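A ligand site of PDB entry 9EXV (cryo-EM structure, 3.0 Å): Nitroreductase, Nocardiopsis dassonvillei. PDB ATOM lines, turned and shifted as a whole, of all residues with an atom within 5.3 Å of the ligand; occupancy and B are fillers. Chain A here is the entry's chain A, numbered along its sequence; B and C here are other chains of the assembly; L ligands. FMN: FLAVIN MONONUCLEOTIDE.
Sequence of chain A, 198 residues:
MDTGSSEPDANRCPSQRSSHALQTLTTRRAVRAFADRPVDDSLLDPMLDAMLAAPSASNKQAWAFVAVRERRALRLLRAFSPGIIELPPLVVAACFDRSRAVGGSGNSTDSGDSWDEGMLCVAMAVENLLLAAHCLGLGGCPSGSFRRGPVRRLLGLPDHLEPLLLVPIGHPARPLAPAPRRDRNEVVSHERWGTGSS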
ATOM      1  N   ARG A  28      -5.985  13.304   2.666  1.00  0.00           N
ATOM      2  CA  ARG A  28      -6.871  12.881   3.743  1.00  0.00           C
ATOM      3  C   ARG A  28      -6.252  13.361   5.050  1.00  0.00           C
ATOM      4  O   ARG A  28      -5.312  12.759   5.573  1.00  0.00           O
ATOM      5  CB  ARG A  28      -7.052  11.365   3.732  1.00  0.00           C
ATOM      6  CG  ARG A  28      -7.892  10.824   4.873  1.00  0.00           C
ATOM      7  CD  ARG A  28      -7.165   9.683   5.589  1.00  0.00           C
ATOM      8  NE  ARG A  28      -6.063  10.185   6.394  1.00  0.00           N
ATOM      9  CZ  ARG A  28      -6.173  10.566   7.655  1.00  0.00           C
ATOM     10  NH1 ARG A  28      -7.325  10.501   8.307  1.00  0.00           N
ATOM     11  NH2 ARG A  28      -5.093  11.029   8.289  1.00  0.00           N
ATOM     12  N   ARG A  29      -6.785  14.465   5.584  1.00  0.00           N
ATOM     13  CA  ARG A  29      -6.294  15.070   6.802  1.00  0.00           C
ATOM     14  C   ARG A  29      -7.327  14.909   7.913  1.00  0.00           C
ATOM     15  O   ARG A  29      -8.532  15.031   7.679  1.00  0.00           O
ATOM     16  CB  ARG A  29      -5.980  16.558   6.596  1.00  0.00           C
ATOM     17  CG  ARG A  29      -4.725  16.829   5.789  1.00  0.00           C
ATOM     18  CD  ARG A  29      -3.481  16.309   6.486  1.00  0.00           C
ATOM     19  NE  ARG A  29      -3.100  14.986   6.009  1.00  0.00           N
ATOM     20  CZ  ARG A  29      -2.467  14.759   4.875  1.00  0.00           C
ATOM     21  NH1 ARG A  29      -2.131  15.751   4.061  1.00  0.00           N
ATOM     22  NH2 ARG A  29      -2.155  13.514   4.534  1.00  0.00           N
ATOM     23  N   ALA A  30      -6.834  14.645   9.125  1.00  0.00           N
ATOM     24  CA  ALA A  30      -7.722  14.489  10.264  1.00  0.00           C
ATOM     25  C   ALA A  30      -8.475  15.786  10.547  1.00  0.00           C
ATOM     26  O   ALA A  30      -7.915  16.875  10.446  1.00  0.00           O
ATOM     27  CB  ALA A  30      -6.929  14.060  11.501  1.00  0.00           C
ATOM     28  N   ARG A  32     -10.736  17.797  13.379  1.00  0.00           N
ATOM     29  CA  ARG A  32     -11.057  17.889  14.792  1.00  0.00           C
ATOM     30  C   ARG A  32     -11.993  19.042  15.139  1.00  0.00           C
ATOM     31  O   ARG A  32     -12.301  19.237  16.322  1.00  0.00           O
ATOM     32  CB  ARG A  32      -9.775  18.029  15.633  1.00  0.00           C
ATOM     33  CG  ARG A  32      -8.880  16.803  15.581  1.00  0.00           C
ATOM     34  CD  ARG A  32      -7.583  17.033  16.337  1.00  0.00           C
ATOM     35  NE  ARG A  32      -6.642  15.945  16.076  1.00  0.00           N
ATOM     36  CZ  ARG A  32      -5.926  15.831  14.967  1.00  0.00           C
ATOM     37  NH1 ARG A  32      -5.955  16.758  14.030  1.00  0.00           N
ATOM     38  NH2 ARG A  32      -5.169  14.744  14.800  1.00  0.00           N
ATOM     39  N   GLY A  83      -9.992  11.725  23.802  1.00  0.00           N
ATOM     40  CA  GLY A  83      -9.528  11.815  22.425  1.00  0.00           C
ATOM     41  C   GLY A  83     -10.343  12.783  21.589  1.00  0.00           C
ATOM     42  O   GLY A  83      -9.806  13.487  20.730  1.00  0.00           O
ATOM     43  N   ILE A  85     -12.115  16.048  20.545  1.00  0.00           N
ATOM     44  CA  ILE A  85     -11.841  17.447  20.829  1.00  0.00           C
ATOM     45  C   ILE A  85     -13.095  18.303  20.694  1.00  0.00           C
ATOM     46  O   ILE A  85     -13.357  19.153  21.542  1.00  0.00           O
ATOM     47  CB  ILE A  85     -10.706  17.943  19.904  1.00  0.00           C
ATOM     48  CG1 ILE A  85      -9.505  17.002  19.990  1.00  0.00           C
ATOM     49  CG2 ILE A  85     -10.308  19.359  20.252  1.00  0.00           C
ATOM     50  CD1 ILE A  85      -8.979  16.808  21.405  1.00  0.00           C
ATOM     51  N   CYS A 141     -11.002  11.781  12.726  1.00  0.00           N
ATOM     52  CA  CYS A 141      -9.714  11.226  13.124  1.00  0.00           C
ATOM     53  C   CYS A 141      -9.923   9.881  13.810  1.00  0.00           C
ATOM     54  O   CYS A 141     -10.937   9.677  14.471  1.00  0.00           O
ATOM     55  CB  CYS A 141      -8.971  12.179  14.081  1.00  0.00           C
ATOM     56  SG  CYS A 141      -9.925  12.646  15.546  1.00  0.00           S
ATOM     57  N   PRO A 142      -8.994   8.937  13.642  1.00  0.00           N
ATOM     58  CA  PRO A 142      -9.119   7.652  14.366  1.00  0.00           C
ATOM     59  C   PRO A 142      -8.770   7.764  15.842  1.00  0.00           C
ATOM     60  O   PRO A 142      -7.805   7.180  16.339  1.00  0.00           O
ATOM     61  CB  PRO A 142      -8.142   6.742  13.604  1.00  0.00           C
ATOM     62  CG  PRO A 142      -7.936   7.385  12.293  1.00  0.00           C
ATOM     63  CD  PRO A 142      -8.018   8.844  12.529  1.00  0.00           C
ATOM     64  N   SER A 143      -9.580   8.516  16.584  1.00  0.00           N
ATOM     65  CA  SER A 143      -9.344   8.670  18.015  1.00  0.00           C
ATOM     66  C   SER A 143      -9.401   7.312  18.700  1.00  0.00           C
ATOM     67  O   SER A 143     -10.288   6.502  18.435  1.00  0.00           O
ATOM     68  CB  SER A 143     -10.382   9.617  18.623  1.00  0.00           C
ATOM     69  OG  SER A 143     -10.220   9.704  20.024  1.00  0.00           O
ATOM     70  N   GLY A 144      -8.431   7.056  19.576  1.00  0.00           N
ATOM     71  CA  GLY A 144      -8.369   5.789  20.287  1.00  0.00           C
ATOM     72  C   GLY A 144      -8.011   5.925  21.750  1.00  0.00           C
ATOM     73  O   GLY A 144      -7.904   4.929  22.469  1.00  0.00           O
ATOM     74  N   SER A 145      -7.803   7.166  22.194  1.00  0.00           N
ATOM     75  CA  SER A 145      -7.447   7.443  23.589  1.00  0.00           C
ATOM     76  C   SER A 145      -8.732   7.698  24.369  1.00  0.00           C
ATOM     77  O   SER A 145      -9.214   8.821  24.463  1.00  0.00           O
ATOM     78  CB  SER A 145      -6.496   8.622  23.673  1.00  0.00           C
ATOM     79  OG  SER A 145      -6.191   8.933  25.018  1.00  0.00           O
ATOM     80  N   LEU A 165     -11.379   1.575  18.685  1.00  0.00           N
ATOM     81  CA  LEU A 165     -11.305   2.936  18.181  1.00  0.00           C
ATOM     82  C   LEU A 165     -12.670   3.597  18.289  1.00  0.00           C
ATOM     83  O   LEU A 165     -13.710   2.924  18.270  1.00  0.00           O
ATOM     84  CB  LEU A 165     -10.805   2.970  16.730  1.00  0.00           C
ATOM     85  CG  LEU A 165      -9.326   2.611  16.562  1.00  0.00           C
ATOM     86  CD1 LEU A 165      -8.996   2.246  15.128  1.00  0.00           C
ATOM     87  CD2 LEU A 165      -8.452   3.770  17.023  1.00  0.00           C
ATOM     88  N   ALA A 179       0.133  18.563   8.048  1.00  0.00           N
ATOM     89  CA  ALA A 179       1.010  18.435   9.205  1.00  0.00           C
ATOM     90  C   ALA A 179       2.427  18.065   8.772  1.00  0.00           C
ATOM     91  O   ALA A 179       2.607  17.373   7.760  1.00  0.00           O
ATOM     92  CB  ALA A 179       0.488  17.385  10.187  1.00  0.00           C
ATOM     93  N   ARG A 181       5.824  16.112   8.242  1.00  0.00           N
ATOM     94  CA  ARG A 181       6.081  14.692   8.097  1.00  0.00           C
ATOM     95  C   ARG A 181       7.585  14.442   8.061  1.00  0.00           C
ATOM     96  O   ARG A 181       8.358  15.285   7.612  1.00  0.00           O
ATOM     97  CB  ARG A 181       5.431  14.133   6.828  1.00  0.00           C
ATOM     98  CG  ARG A 181       5.555  12.620   6.646  1.00  0.00           C
ATOM     99  CD  ARG A 181       5.023  12.180   5.286  1.00  0.00           C
ATOM    100  NE  ARG A 181       3.969  13.079   4.818  1.00  0.00           N
ATOM    101  CZ  ARG A 181       2.754  13.130   5.333  1.00  0.00           C
ATOM    102  NH1 ARG A 181       2.389  12.343   6.336  1.00  0.00           N
ATOM    103  NH2 ARG A 181       1.883  14.014   4.852  1.00  0.00           N
ATOM    104  N   ALA B  53       0.914   8.728   3.530  1.00  0.00           N
ATOM    105  CA  ALA B  53      -0.075   9.730   3.922  1.00  0.00           C
ATOM    106  C   ALA B  53      -1.192   9.051   4.719  1.00  0.00           C
ATOM    107  O   ALA B  53      -2.354   8.989   4.313  1.00  0.00           O
ATOM    108  CB  ALA B  53      -0.612  10.461   2.705  1.00  0.00           C
ATOM    109  N   ALA B  54      -0.807   8.538   5.891  1.00  0.00           N
ATOM    110  CA  ALA B  54      -1.724   7.839   6.768  1.00  0.00           C
ATOM    111  C   ALA B  54      -1.622   8.399   8.177  1.00  0.00           C
ATOM    112  O   ALA B  54      -0.558   8.887   8.577  1.00  0.00           O
ATOM    113  CB  ALA B  54      -1.415   6.332   6.802  1.00  0.00           C
ATOM    114  N   PRO B  55      -2.701   8.336   8.954  1.00  0.00           N
ATOM    115  CA  PRO B  55      -2.656   8.844  10.327  1.00  0.00           C
ATOM    116  C   PRO B  55      -1.712   8.030  11.200  1.00  0.00           C
ATOM    117  O   PRO B  55      -1.530   6.823  11.005  1.00  0.00           O
ATOM    118  CB  PRO B  55      -4.108   8.730  10.805  1.00  0.00           C
ATOM    119  CG  PRO B  55      -4.700   7.673   9.944  1.00  0.00           C
ATOM    120  CD  PRO B  55      -4.027   7.798   8.612  1.00  0.00           C
ATOM    121  N   SER B  56      -1.115   8.706  12.162  1.00  0.00           N
ATOM    122  CA  SER B  56      -0.195   8.126  13.129  1.00  0.00           C
ATOM    123  C   SER B  56      -0.761   8.301  14.528  1.00  0.00           C
ATOM    124  O   SER B  56      -1.851   8.840  14.720  1.00  0.00           O
ATOM    125  CB  SER B  56       1.188   8.768  13.017  1.00  0.00           C
ATOM    126  OG  SER B  56       1.179  10.074  13.525  1.00  0.00           O
ATOM    127  N   ALA B  57      -0.012   7.840  15.533  1.00  0.00           N
ATOM    128  CA  ALA B  57      -0.459   8.016  16.907  1.00  0.00           C
ATOM    129  C   ALA B  57      -0.444   9.489  17.302  1.00  0.00           C
ATOM    130  O   ALA B  57      -1.463  10.033  17.758  1.00  0.00           O
ATOM    131  CB  ALA B  57       0.417   7.190  17.863  1.00  0.00           C
ATOM    132  N   SER B  58       0.704  10.158  17.146  1.00  0.00           N
ATOM    133  CA  SER B  58       0.855  11.539  17.589  1.00  0.00           C
ATOM    134  C   SER B  58       1.696  12.339  16.602  1.00  0.00           C
ATOM    135  O   SER B  58       2.584  13.095  16.996  1.00  0.00           O
ATOM    136  CB  SER B  58       1.486  11.592  18.979  1.00  0.00           C
ATOM    137  OG  SER B  58       1.456  12.920  19.495  1.00  0.00           O
ATOM    138  N   ASN B  59       1.421  12.188  15.300  1.00  0.00           N
ATOM    139  CA  ASN B  59       2.284  12.755  14.263  1.00  0.00           C
ATOM    140  C   ASN B  59       3.745  12.348  14.492  1.00  0.00           C
ATOM    141  O   ASN B  59       4.681  13.049  14.124  1.00  0.00           O
ATOM    142  CB  ASN B  59       2.151  14.277  14.173  1.00  0.00           C
ATOM    143  CG  ASN B  59       2.881  14.851  12.974  1.00  0.00           C
ATOM    144  OD1 ASN B  59       3.432  14.115  12.154  1.00  0.00           O
ATOM    145  ND2 ASN B  59       2.870  16.172  12.852  1.00  0.00           N
ATOM    146  N   GLU B 117      -0.963   1.213  20.971  1.00  0.00           N
ATOM    147  CA  GLU B 117      -1.984   1.918  20.201  1.00  0.00           C
ATOM    148  C   GLU B 117      -1.468   2.281  18.811  1.00  0.00           C
ATOM    149  O   GLU B 117      -2.172   2.094  17.812  1.00  0.00           O
ATOM    150  CB  GLU B 117      -2.439   3.159  20.949  1.00  0.00           C
ATOM    151  CG  GLU B 117      -3.124   4.214  20.095  1.00  0.00           C
ATOM    152  CD  GLU B 117      -3.473   5.469  20.876  1.00  0.00           C
ATOM    153  OE1 GLU B 117      -3.594   5.372  22.119  1.00  0.00           O
ATOM    154  OE2 GLU B 117      -3.610   6.544  20.260  1.00  0.00           O
ATOM    155  N   GLY B 118      -0.243   2.796  18.736  1.00  0.00           N
ATOM    156  CA  GLY B 118       0.311   3.209  17.457  1.00  0.00           C
ATOM    157  C   GLY B 118       0.496   2.074  16.481  1.00  0.00           C
ATOM    158  O   GLY B 118       0.593   2.317  15.269  1.00  0.00           O
ATOM    159  N   LEU B 120      -1.676   0.120  15.502  1.00  0.00           N
ATOM    160  CA  LEU B 120      -2.829   0.148  14.619  1.00  0.00           C
ATOM    161  C   LEU B 120      -2.621   1.123  13.455  1.00  0.00           C
ATOM    162  O   LEU B 120      -3.106   0.872  12.350  1.00  0.00           O
ATOM    163  CB  LEU B 120      -4.085   0.530  15.399  1.00  0.00           C
ATOM    164  CG  LEU B 120      -4.603  -0.449  16.448  1.00  0.00           C
ATOM    165  CD1 LEU B 120      -5.946  -0.001  16.991  1.00  0.00           C
ATOM    166  CD2 LEU B 120      -4.702  -1.853  15.878  1.00  0.00           C
ATOM    167  N   CYS B 121      -1.923   2.228  13.693  1.00  0.00           N
ATOM    168  CA  CYS B 121      -1.710   3.212  12.638  1.00  0.00           C
ATOM    169  C   CYS B 121      -0.894   2.647  11.495  1.00  0.00           C
ATOM    170  O   CYS B 121      -1.111   3.015  10.329  1.00  0.00           O
ATOM    171  CB  CYS B 121      -1.039   4.458  13.223  1.00  0.00           C
ATOM    172  SG  CYS B 121      -2.006   5.274  14.514  1.00  0.00           S
ATOM    173  N   MET B 124      -3.198   0.867   9.396  1.00  0.00           N
ATOM    174  CA  MET B 124      -3.948   1.851   8.615  1.00  0.00           C
ATOM    175  C   MET B 124      -3.159   2.283   7.386  1.00  0.00           C
ATOM    176  O   MET B 124      -3.724   2.395   6.294  1.00  0.00           O
ATOM    177  CB  MET B 124      -4.275   3.065   9.487  1.00  0.00           C
ATOM    178  CG  MET B 124      -5.494   2.881  10.365  1.00  0.00           C
ATOM    179  SD  MET B 124      -5.773   4.278  11.468  1.00  0.00           S
ATOM    180  CE  MET B 124      -6.132   3.413  12.994  1.00  0.00           C
ATOM    181  N   MET C  77      -1.218  19.230  14.665  1.00  0.00           N
ATOM    182  CA  MET C  77      -0.392  18.925  15.827  1.00  0.00           C
ATOM    183  C   MET C  77       1.059  18.785  15.398  1.00  0.00           C
ATOM    184  O   MET C  77       1.360  18.247  14.329  1.00  0.00           O
ATOM    185  CB  MET C  77      -0.857  17.664  16.553  1.00  0.00           C
ATOM    186  CG  MET C  77      -1.334  16.523  15.678  1.00  0.00           C
ATOM    187  SD  MET C  77      -2.460  15.509  16.677  1.00  0.00           S
ATOM    188  CE  MET C  77      -1.296  14.581  17.670  1.00  0.00           C
HETATM  189  N1  FMN L   1      -6.116  12.130  17.078  1.00  0.00           N
HETATM  190  C2  FMN L   1      -6.642  12.833  18.140  1.00  0.00           C
HETATM  191  O2  FMN L   1      -6.878  14.035  18.039  1.00  0.00           O
HETATM  192  N3  FMN L   1      -6.911  12.202  19.341  1.00  0.00           N
HETATM  193  C4  FMN L   1      -6.645  10.863  19.478  1.00  0.00           C
HETATM  194  O4  FMN L   1      -6.879  10.293  20.541  1.00  0.00           O
HETATM  195  C4A FMN L   1      -6.114  10.147  18.412  1.00  0.00           C
HETATM  196  N5  FMN L   1      -5.855   8.810  18.560  1.00  0.00           N
HETATM  197  C5A FMN L   1      -5.319   8.096  17.515  1.00  0.00           C
HETATM  198  C6  FMN L   1      -5.072   6.741  17.700  1.00  0.00           C
HETATM  199  C7  FMN L   1      -4.545   5.979  16.670  1.00  0.00           C
HETATM  200  C7M FMN L   1      -4.297   4.514  16.902  1.00  0.00           C
HETATM  201  C8  FMN L   1      -4.268   6.588  15.450  1.00  0.00           C
HETATM  202  C8M FMN L   1      -3.688   5.796  14.312  1.00  0.00           C
HETATM  203  C9  FMN L   1      -4.523   7.947  15.267  1.00  0.00           C
HETATM  204  C9A FMN L   1      -5.051   8.709  16.297  1.00  0.00           C
HETATM  205  N10 FMN L   1      -5.310  10.075  16.137  1.00  0.00           N
HETATM  206  C10 FMN L   1      -5.845  10.782  17.201  1.00  0.00           C
HETATM  207  C1' FMN L   1      -5.035  10.780  14.844  1.00  0.00           C
HETATM  208  C2' FMN L   1      -3.670  11.480  14.839  1.00  0.00           C
HETATM  209  O2' FMN L   1      -3.662  12.458  15.857  1.00  0.00           O
HETATM  210  C3' FMN L   1      -3.374  12.062  13.449  1.00  0.00           C
HETATM  211  O3' FMN L   1      -2.962  11.003  12.618  1.00  0.00           O
HETATM  212  C4' FMN L   1      -2.297  13.139  13.407  1.00  0.00           C
HETATM  213  O4' FMN L   1      -2.543  14.113  14.361  1.00  0.00           O
HETATM  214  C5' FMN L   1      -2.275  13.880  12.074  1.00  0.00           C
HETATM  215  O5' FMN L   1      -2.159  13.002  10.979  1.00  0.00           O
HETATM  216  P   FMN L   1      -2.361  13.584   9.495  1.00  0.00           P
HETATM  217  O1P FMN L   1      -1.212  14.524   9.201  1.00  0.00           O
HETATM  218  O2P FMN L   1      -2.392  12.458   8.500  1.00  0.00           O
HETATM  219  O3P FMN L   1      -3.665  14.346   9.446  1.00  0.00           O
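The backbone carbonyl oxygen of Pro 142 sits close to a nitrogen (N5) of the ligand. Ser 145 touches the ligand. Ala 179 touches the ligand (CB to O1P, 3.5 Å). Pro 55 of chain B touches the ligand (CB to O3', 3.1 Å). Ala 57 of chain B touches the ligand (O to O2', 3.8 Å). Glu 117 of chain B touches the ligand (OE2 to C6, 3.0 Å). CE of Met 124 of chain B touches C8M of the ligand, 3.7 Å away. Hydrophobic or aromatic side chains that line the ligand: Ala 30, Ala 179, Pro 55 of chain B, Met 124 of chain B and Met 77 of chain C. The nearest printed residue that does not touch the ligand is Ala 54 of chain B (4.02 Å).
The backbone NH (N) of Ala 57 of chain B lies within hydrogen-bond range of the side-chain sulfur (SG) of Cys 121 of chain B. The side-chain sulfur (SD) of Met 77 of chain C lies within hydrogen-bond range of the guanidinium group (NH2) of Arg 32. The side-chain amide nitrogen of Asn 59 of chain B lies within hydrogen-bond range of the backbone carbonyl oxygen of Met 77 of chain C, at 3.0 Å. The side-chain hydroxyl of Ser 56 of chain B sits at hydrogen-bond distance from the backbone NH of Asn 59 of chain B (2.8 Å). The backbone carbonyl oxygen (O) of Ser 145 is in hydrogen-bond range of the backbone NH (N) of Gly 83 (3.1 Å).
A carbon (C8M) of the ligand is bonded to the side-chain sulfur of Cys 121 of chain B. O4' of the ligand lies within hydrogen-bond range of SD of Met 77 of chain C (2.7 Å). NH2 of Arg 32 is in hydrogen-bond range of O4' of the ligand, 2.7 Å away. An oxygen (O3') of the ligand sits at hydrogen-bond distance from the backbone NH of Ser 56 of chain B (3.0 Å). An oxygen (O3') of the ligand lies close to the backbone carbonyl oxygen of Ser 56 of chain B (3.2 Å). NH2 of Arg 28 lies within salt-bridge range of O2P of the ligand (3.1 Å). The backbone NH (N) of Ala 30 lies within hydrogen-bond range of an oxygen (O3P) of the ligand, 3.2 Å away. N5 of the ligand sits at hydrogen-bond distance from N of Gly 144, at 3.3 Å. OG of Ser 143 lies within hydrogen-bond range of O4 of the ligand. A nitrogen (N3) of the ligand lies within hydrogen-bond range of the backbone carbonyl oxygen of Gly 83. The guanidinium group of Arg 29 is in salt-bridge range of an oxygen (O3P) of the ligand (3.5 Å).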
